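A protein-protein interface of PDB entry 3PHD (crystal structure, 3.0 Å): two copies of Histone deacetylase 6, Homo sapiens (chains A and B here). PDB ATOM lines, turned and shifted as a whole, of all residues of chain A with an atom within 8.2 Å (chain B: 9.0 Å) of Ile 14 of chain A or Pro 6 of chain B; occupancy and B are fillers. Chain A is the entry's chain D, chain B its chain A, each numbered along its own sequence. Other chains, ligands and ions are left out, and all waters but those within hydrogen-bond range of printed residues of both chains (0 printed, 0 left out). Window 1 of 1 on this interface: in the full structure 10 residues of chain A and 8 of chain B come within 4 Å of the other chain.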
ATOM      1  N   LEU A   8      -5.791 -23.431  22.080  1.00  0.00           N
ATOM      2  CA  LEU A   8      -5.530 -23.303  20.653  1.00  0.00           C
ATOM      3  C   LEU A   8      -4.939 -24.593  20.051  1.00  0.00           C
ATOM      4  O   LEU A   8      -5.065 -24.792  18.855  1.00  0.00           O
ATOM      5  CB  LEU A   8      -4.668 -22.065  20.341  1.00  0.00           C
ATOM      6  CG  LEU A   8      -5.291 -20.699  20.668  1.00  0.00           C
ATOM      7  CD1 LEU A   8      -4.245 -19.665  20.873  1.00  0.00           C
ATOM      8  CD2 LEU A   8      -6.280 -20.234  19.599  1.00  0.00           C
ATOM      9  N   VAL A   9      -4.349 -25.480  20.880  1.00  0.00           N
ATOM     10  CA  VAL A   9      -3.792 -26.772  20.491  1.00  0.00           C
ATOM     11  C   VAL A   9      -4.857 -27.679  19.814  1.00  0.00           C
ATOM     12  O   VAL A   9      -4.534 -28.476  18.921  1.00  0.00           O
ATOM     13  CB  VAL A   9      -3.106 -27.506  21.682  1.00  0.00           C
ATOM     14  CG1 VAL A   9      -1.916 -26.727  22.198  1.00  0.00           C
ATOM     15  CG2 VAL A   9      -4.085 -27.777  22.825  1.00  0.00           C
ATOM     16  N   ALA A  10      -6.119 -27.554  20.247  1.00  0.00           N
ATOM     17  CA  ALA A  10      -7.240 -28.343  19.740  1.00  0.00           C
ATOM     18  C   ALA A  10      -7.670 -27.993  18.285  1.00  0.00           C
ATOM     19  O   ALA A  10      -8.368 -28.774  17.635  1.00  0.00           O
ATOM     20  CB  ALA A  10      -8.409 -28.194  20.688  1.00  0.00           C
ATOM     21  N   VAL A  11      -7.263 -26.810  17.808  1.00  0.00           N
ATOM     22  CA  VAL A  11      -7.588 -26.274  16.489  1.00  0.00           C
ATOM     23  C   VAL A  11      -7.022 -27.136  15.340  1.00  0.00           C
ATOM     24  O   VAL A  11      -5.892 -27.601  15.408  1.00  0.00           O
ATOM     25  CB  VAL A  11      -7.149 -24.796  16.423  1.00  0.00           C
ATOM     26  CG1 VAL A  11      -6.840 -24.360  15.017  1.00  0.00           C
ATOM     27  CG2 VAL A  11      -8.164 -23.880  17.103  1.00  0.00           C
ATOM     28  N   CYS A  12      -7.831 -27.355  14.301  1.00  0.00           N
ATOM     29  CA  CYS A  12      -7.469 -28.125  13.111  1.00  0.00           C
ATOM     30  C   CYS A  12      -7.321 -27.252  11.853  1.00  0.00           C
ATOM     31  O   CYS A  12      -7.747 -26.097  11.877  1.00  0.00           O
ATOM     32  CB  CYS A  12      -8.492 -29.226  12.894  1.00  0.00           C
ATOM     33  SG  CYS A  12      -8.275 -30.649  13.983  1.00  0.00           S
ATOM     34  N   PRO A  13      -6.730 -27.757  10.744  1.00  0.00           N
ATOM     35  CA  PRO A  13      -6.607 -26.898   9.536  1.00  0.00           C
ATOM     36  C   PRO A  13      -7.956 -26.535   8.876  1.00  0.00           C
ATOM     37  O   PRO A  13      -8.905 -27.326   8.981  1.00  0.00           O
ATOM     38  CB  PRO A  13      -5.734 -27.731   8.576  1.00  0.00           C
ATOM     39  CG  PRO A  13      -5.690 -29.092   9.121  1.00  0.00           C
ATOM     40  CD  PRO A  13      -6.153 -29.103  10.533  1.00  0.00           C
ATOM     41  N   ILE A  14      -8.047 -25.370   8.199  1.00  0.00           N
ATOM     42  CA  ILE A  14      -9.274 -24.991   7.485  1.00  0.00           C
ATOM     43  C   ILE A  14      -9.513 -26.048   6.383  1.00  0.00           C
ATOM     44  O   ILE A  14      -8.579 -26.378   5.648  1.00  0.00           O
ATOM     45  CB  ILE A  14      -9.249 -23.548   6.860  1.00  0.00           C
ATOM     46  CG2 ILE A  14      -9.039 -22.430   7.909  1.00  0.00           C
ATOM     47  N   PRO A  15     -10.717 -26.649   6.301  1.00  0.00           N
ATOM     48  CA  PRO A  15     -10.977 -27.640   5.242  1.00  0.00           C
ATOM     49  C   PRO A  15     -10.719 -27.115   3.817  1.00  0.00           C
ATOM     50  O   PRO A  15     -10.893 -25.919   3.547  1.00  0.00           O
ATOM     51  CB  PRO A  15     -12.474 -27.936   5.426  1.00  0.00           C
ATOM     52  CG  PRO A  15     -12.779 -27.558   6.800  1.00  0.00           C
ATOM     53  CD  PRO A  15     -11.936 -26.382   7.085  1.00  0.00           C
ATOM     54  N   ALA A  16     -10.351 -28.024   2.892  1.00  0.00           N
ATOM     55  CA  ALA A  16     -10.100 -27.707   1.473  1.00  0.00           C
ATOM     56  C   ALA A  16     -11.235 -26.872   0.870  1.00  0.00           C
ATOM     57  O   ALA A  16     -10.978 -25.857   0.205  1.00  0.00           O
ATOM     58  CB  ALA A  16      -9.909 -28.985   0.669  1.00  0.00           C
ATOM     59  N   ALA A  17     -12.489 -27.252   1.202  1.00  0.00           N
ATOM     60  CA  ALA A  17     -13.701 -26.550   0.765  1.00  0.00           C
ATOM     61  C   ALA A  17     -13.799 -25.082   1.256  1.00  0.00           C
ATOM     62  O   ALA A  17     -14.506 -24.288   0.636  1.00  0.00           O
ATOM     63  CB  ALA A  17     -14.925 -27.327   1.204  1.00  0.00           C
ATOM     64  N   GLY A  18     -13.068 -24.745   2.327  1.00  0.00           N
ATOM     65  CA  GLY A  18     -13.063 -23.424   2.949  1.00  0.00           C
ATOM     66  C   GLY A  18     -14.207 -23.262   3.933  1.00  0.00           C
ATOM     67  O   GLY A  18     -14.925 -24.226   4.232  1.00  0.00           O
ATOM     68  N   LEU A  19     -14.404 -22.037   4.433  1.00  0.00           N
ATOM     69  CA  LEU A  19     -15.501 -21.748   5.358  1.00  0.00           C
ATOM     70  C   LEU A  19     -16.650 -21.029   4.639  1.00  0.00           C
ATOM     71  O   LEU A  19     -16.394 -20.184   3.780  1.00  0.00           O
ATOM     72  CB  LEU A  19     -15.004 -20.909   6.539  1.00  0.00           C
ATOM     73  CG  LEU A  19     -13.829 -21.462   7.343  1.00  0.00           C
ATOM     74  CD1 LEU A  19     -13.420 -20.473   8.455  1.00  0.00           C
ATOM     75  CD2 LEU A  19     -14.120 -22.872   7.903  1.00  0.00           C
ATOM     76  N   CYS A  37     -17.005 -24.590  14.444  1.00  0.00           N
ATOM     77  CA  CYS A  37     -16.078 -25.228  15.365  1.00  0.00           C
ATOM     78  C   CYS A  37     -14.700 -25.305  14.677  1.00  0.00           C
ATOM     79  O   CYS A  37     -14.602 -25.820  13.564  1.00  0.00           O
ATOM     80  CB  CYS A  37     -16.591 -26.609  15.761  1.00  0.00           C
ATOM     81  SG  CYS A  37     -15.424 -27.562  16.761  1.00  0.00           S
ATOM     82  N   LEU A  38     -13.643 -24.788  15.329  1.00  0.00           N
ATOM     83  CA  LEU A  38     -12.289 -24.803  14.763  1.00  0.00           C
ATOM     84  C   LEU A  38     -11.541 -26.129  14.880  1.00  0.00           C
ATOM     85  O   LEU A  38     -10.386 -26.210  14.466  1.00  0.00           O
ATOM     86  CB  LEU A  38     -11.433 -23.635  15.275  1.00  0.00           C
ATOM     87  CG  LEU A  38     -11.997 -22.223  15.061  1.00  0.00           C
ATOM     88  CD1 LEU A  38     -11.082 -21.214  15.674  1.00  0.00           C
ATOM     89  CD2 LEU A  38     -12.196 -21.910  13.565  1.00  0.00           C
ATOM     90  N   SER A  39     -12.212 -27.179  15.381  1.00  0.00           N
ATOM     91  CA  SER A  39     -11.617 -28.510  15.479  1.00  0.00           C
ATOM     92  C   SER A  39     -12.231 -29.454  14.463  1.00  0.00           C
ATOM     93  O   SER A  39     -11.499 -30.243  13.862  1.00  0.00           O
ATOM     94  CB  SER A  39     -11.777 -29.079  16.889  1.00  0.00           C
ATOM     95  OG  SER A  39     -11.224 -28.217  17.869  1.00  0.00           O
ATOM     96  N   TYR A  41     -14.984 -28.267  12.295  1.00  0.00           N
ATOM     97  CA  TYR A  41     -15.575 -27.399  11.279  1.00  0.00           C
ATOM     98  C   TYR A  41     -17.078 -27.550  11.016  1.00  0.00           C
ATOM     99  O   TYR A  41     -17.579 -27.119   9.978  1.00  0.00           O
ATOM    100  CB  TYR A  41     -14.675 -27.295  10.026  1.00  0.00           C
ATOM    101  CG  TYR A  41     -13.379 -26.581  10.334  1.00  0.00           C
ATOM    102  CD1 TYR A  41     -13.302 -25.194  10.305  1.00  0.00           C
ATOM    103  CD2 TYR A  41     -12.256 -27.285  10.746  1.00  0.00           C
ATOM    104  CE1 TYR A  41     -12.122 -24.522  10.645  1.00  0.00           C
ATOM    105  CE2 TYR A  41     -11.077 -26.628  11.106  1.00  0.00           C
ATOM    106  CZ  TYR A  41     -11.006 -25.247  11.037  1.00  0.00           C
ATOM    107  OH  TYR A  41      -9.835 -24.610  11.381  1.00  0.00           O
ATOM    108  N   LEU A  64     -12.727 -24.215  20.849  1.00  0.00           N
ATOM    109  CA  LEU A  64     -12.745 -22.976  20.086  1.00  0.00           C
ATOM    110  C   LEU A  64     -13.670 -22.923  18.944  1.00  0.00           C
ATOM    111  O   LEU A  64     -13.622 -23.770  18.054  1.00  0.00           O
ATOM    112  CB  LEU A  64     -11.330 -22.557  19.676  1.00  0.00           C
ATOM    113  CG  LEU A  64     -10.514 -22.035  20.811  1.00  0.00           C
ATOM    114  CD1 LEU A  64      -9.147 -22.598  20.749  1.00  0.00           C
ATOM    115  CD2 LEU A  64     -10.560 -20.524  20.863  1.00  0.00           C
ATOM    116  N   LEU A  66     -15.678 -20.014  16.121  1.00  0.00           N
ATOM    117  CA  LEU A  66     -15.588 -18.753  15.411  1.00  0.00           C
ATOM    118  C   LEU A  66     -16.967 -18.302  14.965  1.00  0.00           C
ATOM    119  O   LEU A  66     -17.650 -19.055  14.258  1.00  0.00           O
ATOM    120  CB  LEU A  66     -14.703 -18.988  14.176  1.00  0.00           C
ATOM    121  CG  LEU A  66     -14.224 -17.770  13.396  1.00  0.00           C
ATOM    122  CD1 LEU A  66     -13.179 -16.976  14.195  1.00  0.00           C
ATOM    123  CD2 LEU A  66     -13.658 -18.206  12.070  1.00  0.00           C
ATOM    124  N   HIS A  83      -8.999 -14.113  20.253  1.00  0.00           N
ATOM    125  CA  HIS A  83      -8.398 -13.200  19.302  1.00  0.00           C
ATOM    126  C   HIS A  83      -9.488 -12.747  18.369  1.00  0.00           C
ATOM    127  O   HIS A  83     -10.614 -13.250  18.446  1.00  0.00           O
ATOM    128  CB  HIS A  83      -7.186 -13.814  18.555  1.00  0.00           C
ATOM    129  CG  HIS A  83      -7.445 -15.137  17.890  1.00  0.00           C
ATOM    130  ND1 HIS A  83      -8.129 -15.223  16.683  1.00  0.00           N
ATOM    131  CD2 HIS A  83      -7.061 -16.382  18.262  1.00  0.00           C
ATOM    132  CE1 HIS A  83      -8.167 -16.511  16.382  1.00  0.00           C
ATOM    133  NE2 HIS A  83      -7.533 -17.249  17.298  1.00  0.00           N
ATOM    134  N   GLN A  85      -8.860 -12.242  14.743  1.00  0.00           N
ATOM    135  CA  GLN A  85      -8.216 -12.488  13.447  1.00  0.00           C
ATOM    136  C   GLN A  85      -9.209 -13.314  12.545  1.00  0.00           C
ATOM    137  O   GLN A  85      -9.882 -14.241  13.046  1.00  0.00           O
ATOM    138  CB  GLN A  85      -6.892 -13.230  13.668  1.00  0.00           C
ATOM    139  CG  GLN A  85      -6.097 -12.792  14.901  1.00  0.00           C
ATOM    140  N   LEU A  87     -10.797 -14.563   8.185  1.00  0.00           N
ATOM    141  CA  LEU A  87     -10.899 -14.855   6.761  1.00  0.00           C
ATOM    142  C   LEU A  87     -11.696 -13.798   5.986  1.00  0.00           C
ATOM    143  O   LEU A  87     -12.287 -14.106   4.943  1.00  0.00           O
ATOM    144  CB  LEU A  87     -11.580 -16.230   6.575  1.00  0.00           C
ATOM    145  CG  LEU A  87     -10.774 -17.527   6.832  1.00  0.00           C
ATOM    146  CD1 LEU A  87     -11.183 -18.620   5.847  1.00  0.00           C
ATOM    147  CD2 LEU A  87      -9.294 -17.327   6.676  1.00  0.00           C
ATOM    148  N   LEU B   2      -4.649 -18.273   1.788  1.00  0.00           N
ATOM    149  CA  LEU B   2      -5.503 -17.889   2.917  1.00  0.00           C
ATOM    150  C   LEU B   2      -5.240 -16.500   3.540  1.00  0.00           C
ATOM    151  O   LEU B   2      -4.095 -16.126   3.819  1.00  0.00           O
ATOM    152  CB  LEU B   2      -5.453 -18.957   4.023  1.00  0.00           C
ATOM    153  CG  LEU B   2      -5.901 -20.386   3.695  1.00  0.00           C
ATOM    154  CD1 LEU B   2      -5.368 -21.356   4.721  1.00  0.00           C
ATOM    155  CD2 LEU B   2      -7.393 -20.499   3.699  1.00  0.00           C
ATOM    156  N   PRO B   3      -6.323 -15.763   3.873  1.00  0.00           N
ATOM    157  CA  PRO B   3      -6.150 -14.445   4.522  1.00  0.00           C
ATOM    158  C   PRO B   3      -5.888 -14.552   6.016  1.00  0.00           C
ATOM    159  O   PRO B   3      -5.688 -13.543   6.687  1.00  0.00           O
ATOM    160  CB  PRO B   3      -7.493 -13.744   4.275  1.00  0.00           C
ATOM    161  CG  PRO B   3      -8.448 -14.801   4.052  1.00  0.00           C
ATOM    162  CD  PRO B   3      -7.748 -16.070   3.644  1.00  0.00           C
ATOM    163  N   TRP B   4      -5.946 -15.781   6.533  1.00  0.00           N
ATOM    164  CA  TRP B   4      -5.793 -16.194   7.934  1.00  0.00           C
ATOM    165  C   TRP B   4      -5.881 -17.733   7.970  1.00  0.00           C
ATOM    166  O   TRP B   4      -6.508 -18.344   7.096  1.00  0.00           O
ATOM    167  CB  TRP B   4      -6.910 -15.579   8.806  1.00  0.00           C
ATOM    168  CG  TRP B   4      -6.967 -16.073  10.226  1.00  0.00           C
ATOM    169  CD1 TRP B   4      -6.327 -15.533  11.304  1.00  0.00           C
ATOM    170  CD2 TRP B   4      -7.748 -17.180  10.733  1.00  0.00           C
ATOM    171  NE1 TRP B   4      -6.661 -16.226  12.451  1.00  0.00           N
ATOM    172  CE2 TRP B   4      -7.518 -17.252  12.126  1.00  0.00           C
ATOM    173  CE3 TRP B   4      -8.608 -18.130  10.141  1.00  0.00           C
ATOM    174  CZ2 TRP B   4      -8.123 -18.226  12.935  1.00  0.00           C
ATOM    175  CZ3 TRP B   4      -9.207 -19.087  10.944  1.00  0.00           C
ATOM    176  CH2 TRP B   4      -8.953 -19.138  12.318  1.00  0.00           C
ATOM    177  N   CYS B   5      -5.231 -18.343   8.977  1.00  0.00           N
ATOM    178  CA  CYS B   5      -5.256 -19.774   9.248  1.00  0.00           C
ATOM    179  C   CYS B   5      -5.137 -19.950  10.768  1.00  0.00           C
ATOM    180  O   CYS B   5      -4.600 -19.072  11.466  1.00  0.00           O
ATOM    181  CB  CYS B   5      -4.193 -20.545   8.460  1.00  0.00           C
ATOM    182  SG  CYS B   5      -2.711 -21.000   9.390  1.00  0.00           S
ATOM    183  N   PRO B   6      -5.691 -21.036  11.326  1.00  0.00           N
ATOM    184  CA  PRO B   6      -5.681 -21.174  12.787  1.00  0.00           C
ATOM    185  C   PRO B   6      -4.320 -21.471  13.421  1.00  0.00           C
ATOM    186  O   PRO B   6      -4.227 -21.622  14.644  1.00  0.00           O
ATOM    187  CB  PRO B   6      -6.703 -22.272  13.020  1.00  0.00           C
ATOM    188  CG  PRO B   6      -6.721 -23.058  11.804  1.00  0.00           C
ATOM    189  CD  PRO B   6      -6.441 -22.132  10.681  1.00  0.00           C
ATOM    190  N   HIS B   7      -3.257 -21.522  12.602  1.00  0.00           N
ATOM    191  CA  HIS B   7      -1.913 -21.843  13.067  1.00  0.00           C
ATOM    192  C   HIS B   7      -1.006 -20.646  13.226  1.00  0.00           C
ATOM    193  O   HIS B   7       0.077 -20.798  13.767  1.00  0.00           O
ATOM    194  CB  HIS B   7      -1.288 -22.962  12.216  1.00  0.00           C
ATOM    195  CG  HIS B   7      -2.182 -24.156  12.077  1.00  0.00           C
ATOM    196  ND1 HIS B   7      -2.952 -24.353  10.937  1.00  0.00           N
ATOM    197  CD2 HIS B   7      -2.461 -25.132  12.968  1.00  0.00           C
ATOM    198  CE1 HIS B   7      -3.647 -25.453  11.163  1.00  0.00           C
ATOM    199  NE2 HIS B   7      -3.371 -25.968  12.368  1.00  0.00           N
ATOM    200  N   LEU B   8      -1.457 -19.438  12.846  1.00  0.00           N
ATOM    201  CA  LEU B   8      -0.662 -18.200  12.988  1.00  0.00           C
ATOM    202  C   LEU B   8      -0.232 -17.920  14.438  1.00  0.00           C
ATOM    203  O   LEU B   8       0.765 -17.245  14.664  1.00  0.00           O
ATOM    204  CB  LEU B   8      -1.399 -16.992  12.387  1.00  0.00           C
ATOM    205  CG  LEU B   8      -1.594 -17.007  10.889  1.00  0.00           C
ATOM    206  CD1 LEU B   8      -2.768 -16.121  10.487  1.00  0.00           C
ATOM    207  CD2 LEU B   8      -0.294 -16.635  10.163  1.00  0.00           C
ATOM    208  N   VAL B   9      -0.964 -18.483  15.404  1.00  0.00           N
ATOM    209  CA  VAL B   9      -0.677 -18.395  16.841  1.00  0.00           C
ATOM    210  C   VAL B   9       0.717 -18.997  17.170  1.00  0.00           C
ATOM    211  O   VAL B   9       1.372 -18.542  18.108  1.00  0.00           O
ATOM    212  CB  VAL B   9      -1.783 -19.067  17.697  1.00  0.00           C
ATOM    213  CG1 VAL B   9      -3.111 -18.349  17.529  1.00  0.00           C
ATOM    214  CG2 VAL B   9      -1.934 -20.560  17.379  1.00  0.00           C
ATOM    215  N   ALA B  10       1.155 -20.014  16.391  1.00  0.00           N
ATOM    216  CA  ALA B  10       2.426 -20.722  16.561  1.00  0.00           C
ATOM    217  C   ALA B  10       3.638 -19.913  16.152  1.00  0.00           C
ATOM    218  O   ALA B  10       4.753 -20.316  16.468  1.00  0.00           O
ATOM    219  CB  ALA B  10       2.410 -22.041  15.814  1.00  0.00           C
ATOM    220  N   VAL B  11       3.446 -18.772  15.481  1.00  0.00           N
ATOM    221  CA  VAL B  11       4.523 -17.868  15.054  1.00  0.00           C
ATOM    222  C   VAL B  11       5.164 -17.166  16.257  1.00  0.00           C
ATOM    223  O   VAL B  11       4.458 -16.528  17.045  1.00  0.00           O
ATOM    224  CB  VAL B  11       3.994 -16.840  14.031  1.00  0.00           C
ATOM    225  CG1 VAL B  11       4.902 -15.623  13.960  1.00  0.00           C
ATOM    226  CG2 VAL B  11       3.829 -17.470  12.652  1.00  0.00           C
ATOM    227  N   PRO B  63       4.043 -25.479  12.298  1.00  0.00           N
ATOM    228  CA  PRO B  63       3.255 -25.330  11.059  1.00  0.00           C
ATOM    229  C   PRO B  63       3.683 -24.300  10.026  1.00  0.00           C
ATOM    230  O   PRO B  63       3.460 -24.526   8.841  1.00  0.00           O
ATOM    231  CB  PRO B  63       1.868 -24.982  11.587  1.00  0.00           C
ATOM    232  CG  PRO B  63       2.124 -24.243  12.827  1.00  0.00           C
ATOM    233  CD  PRO B  63       3.355 -24.849  13.442  1.00  0.00           C
ATOM    234  N   LEU B  64       4.192 -23.139  10.466  1.00  0.00           N
ATOM    235  CA  LEU B  64       4.494 -22.064   9.537  1.00  0.00           C
ATOM    236  C   LEU B  64       5.939 -21.848   9.223  1.00  0.00           C
ATOM    237  O   LEU B  64       6.766 -21.705  10.113  1.00  0.00           O
ATOM    238  CB  LEU B  64       3.796 -20.774   9.938  1.00  0.00           C
ATOM    239  CG  LEU B  64       2.298 -20.806   9.671  1.00  0.00           C
ATOM    240  CD1 LEU B  64       1.552 -20.173  10.763  1.00  0.00           C
ATOM    241  CD2 LEU B  64       1.947 -20.147   8.373  1.00  0.00           C
ATOM    242  N   CYS B  75       1.600 -22.862   5.400  1.00  0.00           N
ATOM    243  CA  CYS B  75       1.150 -23.619   6.569  1.00  0.00           C
ATOM    244  C   CYS B  75       1.012 -25.063   6.138  1.00  0.00           C
ATOM    245  O   CYS B  75       0.214 -25.369   5.238  1.00  0.00           O
ATOM    246  CB  CYS B  75      -0.141 -23.092   7.181  1.00  0.00           C
ATOM    247  SG  CYS B  75      -0.801 -24.167   8.490  1.00  0.00           S
ATOM    248  N   TYR B  77      -0.203 -27.674   7.762  1.00  0.00           N
ATOM    249  CA  TYR B  77      -1.484 -28.300   8.083  1.00  0.00           C
ATOM    250  C   TYR B  77      -2.587 -27.890   7.111  1.00  0.00           C
ATOM    251  O   TYR B  77      -3.279 -28.760   6.545  1.00  0.00           O
ATOM    252  CB  TYR B  77      -1.899 -28.031   9.546  1.00  0.00           C
ATOM    253  CG  TYR B  77      -0.923 -28.615  10.529  1.00  0.00           C
ATOM    254  CD1 TYR B  77      -0.675 -29.985  10.564  1.00  0.00           C
ATOM    255  CD2 TYR B  77      -0.230 -27.801  11.418  1.00  0.00           C
ATOM    256  CE1 TYR B  77       0.234 -30.527  11.459  1.00  0.00           C
ATOM    257  CE2 TYR B  77       0.673 -28.335  12.328  1.00  0.00           C
ATOM    258  CZ  TYR B  77       0.896 -29.700  12.351  1.00  0.00           C
ATOM    259  OH  TYR B  77       1.793 -30.242  13.238  1.00  0.00           O
ATOM    260  N   CYS B  78      -2.728 -26.566   6.911  1.00  0.00           N
ATOM    261  CA  CYS B  78      -3.699 -25.983   6.018  1.00  0.00           C
ATOM    262  C   CYS B  78      -3.352 -26.224   4.574  1.00  0.00           C
ATOM    263  O   CYS B  78      -4.200 -25.984   3.711  1.00  0.00           O
ATOM    264  CB  CYS B  78      -3.864 -24.509   6.315  1.00  0.00           C
ATOM    265  SG  CYS B  78      -4.407 -24.198   7.997  1.00  0.00           S
ATOM    266  N   GLN B  79      -2.120 -26.705   4.298  1.00  0.00           N
ATOM    267  CA  GLN B  79      -1.637 -27.017   2.958  1.00  0.00           C
ATOM    268  C   GLN B  79      -1.933 -25.870   2.008  1.00  0.00           C
ATOM    269  O   GLN B  79      -2.531 -26.068   0.959  1.00  0.00           O
ATOM    270  CB  GLN B  79      -2.207 -28.356   2.469  1.00  0.00           C
ATOM    271  CG  GLN B  79      -1.525 -29.534   3.125  1.00  0.00           C
ATOM    272  CD  GLN B  79      -1.973 -30.853   2.592  1.00  0.00           C
ATOM    273  OE1 GLN B  79      -3.161 -31.203   2.562  1.00  0.00           O
ATOM    274  NE2 GLN B  79      -1.001 -31.647   2.187  1.00  0.00           N
ATOM    275  N   ALA B  80      -1.541 -24.647   2.419  1.00  0.00           N
ATOM    276  CA  ALA B  80      -1.776 -23.400   1.691  1.00  0.00           C
ATOM    277  C   ALA B  80      -0.842 -22.258   2.110  1.00  0.00           C
ATOM    278  O   ALA B  80      -0.386 -22.232   3.253  1.00  0.00           O
ATOM    279  CB  ALA B  80      -3.209 -22.962   1.924  1.00  0.00           C
ATOM    280  N   VAL B  82      -0.258 -18.613   3.465  1.00  0.00           N
ATOM    281  CA  VAL B  82      -1.053 -17.752   4.339  1.00  0.00           C
ATOM    282  C   VAL B  82      -0.478 -16.334   4.274  1.00  0.00           C
ATOM    283  O   VAL B  82       0.740 -16.178   4.317  1.00  0.00           O
ATOM    284  CB  VAL B  82      -1.149 -18.266   5.824  1.00  0.00           C
ATOM    285  CG1 VAL B  82      -2.182 -17.470   6.620  1.00  0.00           C
ATOM    286  CG2 VAL B  82      -1.457 -19.757   5.912  1.00  0.00           C
ATOM    287  N   HIS B  84      -1.156 -12.487   6.239  1.00  0.00           N
ATOM    288  CA  HIS B  84      -1.828 -11.875   7.387  1.00  0.00           C
ATOM    289  C   HIS B  84      -0.903 -10.860   8.100  1.00  0.00           C
ATOM    290  O   HIS B  84       0.307 -10.938   7.943  1.00  0.00           O
ATOM    291  CB  HIS B  84      -2.227 -13.010   8.373  1.00  0.00           C
ATOM    292  CG  HIS B  84      -3.168 -12.613   9.472  1.00  0.00           C
ATOM    293  ND1 HIS B  84      -2.725 -11.923  10.598  1.00  0.00           N
ATOM    294  CD2 HIS B  84      -4.486 -12.876   9.613  1.00  0.00           C
ATOM    295  CE1 HIS B  84      -3.797 -11.730  11.342  1.00  0.00           C
ATOM    296  NE2 HIS B  84      -4.880 -12.294  10.799  1.00  0.00           N
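The backbone carbonyl oxygen (O) of Leu 38 of chain A sits at hydrogen-bond distance from the backbone NH (N) of Cys 12 of chain A (2.8 Å). The backbone carbonyl oxygen (O) of Ser 39 of chain A lies within hydrogen-bond range of the side-chain sulfur (SG) of Cys 12 of chain A. The side-chain sulfur (SG) of Cys 75 of chain B sits close to the backbone NH (N) of Tyr 77 of chain B (3.6 Å). The side-chain hydroxyl (OH) of Tyr 41 of chain A lies within hydrogen-bond range of the backbone carbonyl oxygen (O) of Cys 12 of chain A (2.6 Å).
Among the printed residues, merely in contact across the chains: Leu 8 of chain A with Val 9 of chain B (3.8 Å), Val 11 of chain A with Pro 6 of chain B (2.9 Å), Cys 12 of chain A with Pro 6 of chain B (3.2 Å), Pro 13 of chain A with His 7 of chain B (3.7 Å), Pro 13 of chain A with Tyr 77 of chain B (3.3 Å), Pro 13 of chain A with Cys 78 of chain B (3.6 Å), Ile 14 of chain A with Pro 6 of chain B (3.8 Å), Ile 14 of chain A with Cys 78 of chain B (3.8 Å), Tyr 41 of chain A with Pro 6 of chain B (3.5 Å), His 83 of chain A with Trp 4 of chain B (3.9 Å), Gln 85 of chain A with Trp 4 of chain B (3.2 Å), Gln 85 of chain A with His 84 of chain B (3.6 Å), Leu 87 of chain A with Pro 3 of chain B (3.6 Å) and Leu 87 of chain A with Trp 4 of chain B (3.0 Å).
Of the printed residues of chain B, Ile 14 of chain A touches Pro 6 and Cys 78. Of chain A, only Val 11 (2.9 Å), Cys 12 (3.2 Å), Ile 14 (3.8 Å) and Tyr 41 (3.5 Å) come within 4 Å of Pro 6 of chain B. No residue of chain A comes within 4 Å of Cys 5 of chain B. Printed residues of chain A within 4 Å of Pro 3 of chain B: Leu 87 (3.6 Å). Of the printed residues of chain B, Cys 12 of chain A touches Pro 6 (3.2 Å). Ala 10 of chain B touches none of the printed residues of chain A. Pro 63 of chain B touches none of the printed residues of chain A. The nearest residue of chain B that does not touch Ile 14 of chain A is Trp 4 of chain B (4.5 Å). The nearest residue of chain A that does not touch Pro 6 of chain B is Pro 13 of chain A (4.5 Å). The nearest printed residue of chain A that does not touch Tyr 77 of chain B is Ile 14 of chain A (5.9 Å).
Hydrophobic or aromatic side chains of chain B within 4 Å of the printed part of chain A: Pro 3, Trp 4, Pro 6, His 7, Val 9, Tyr 77 and His 84. Among the printed residues, 14 pairs touch across the chains. Among the printed residues, no Asp or Glu carboxylate lies within 4 Å of a Lys or Arg side-chain nitrogen of the other chain.
Leu 8 of chain A touches Val 9 of chain B, but with the chains exchanged Val 9 of chain A does not touch Leu 8 of chain B (10.5 Å).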
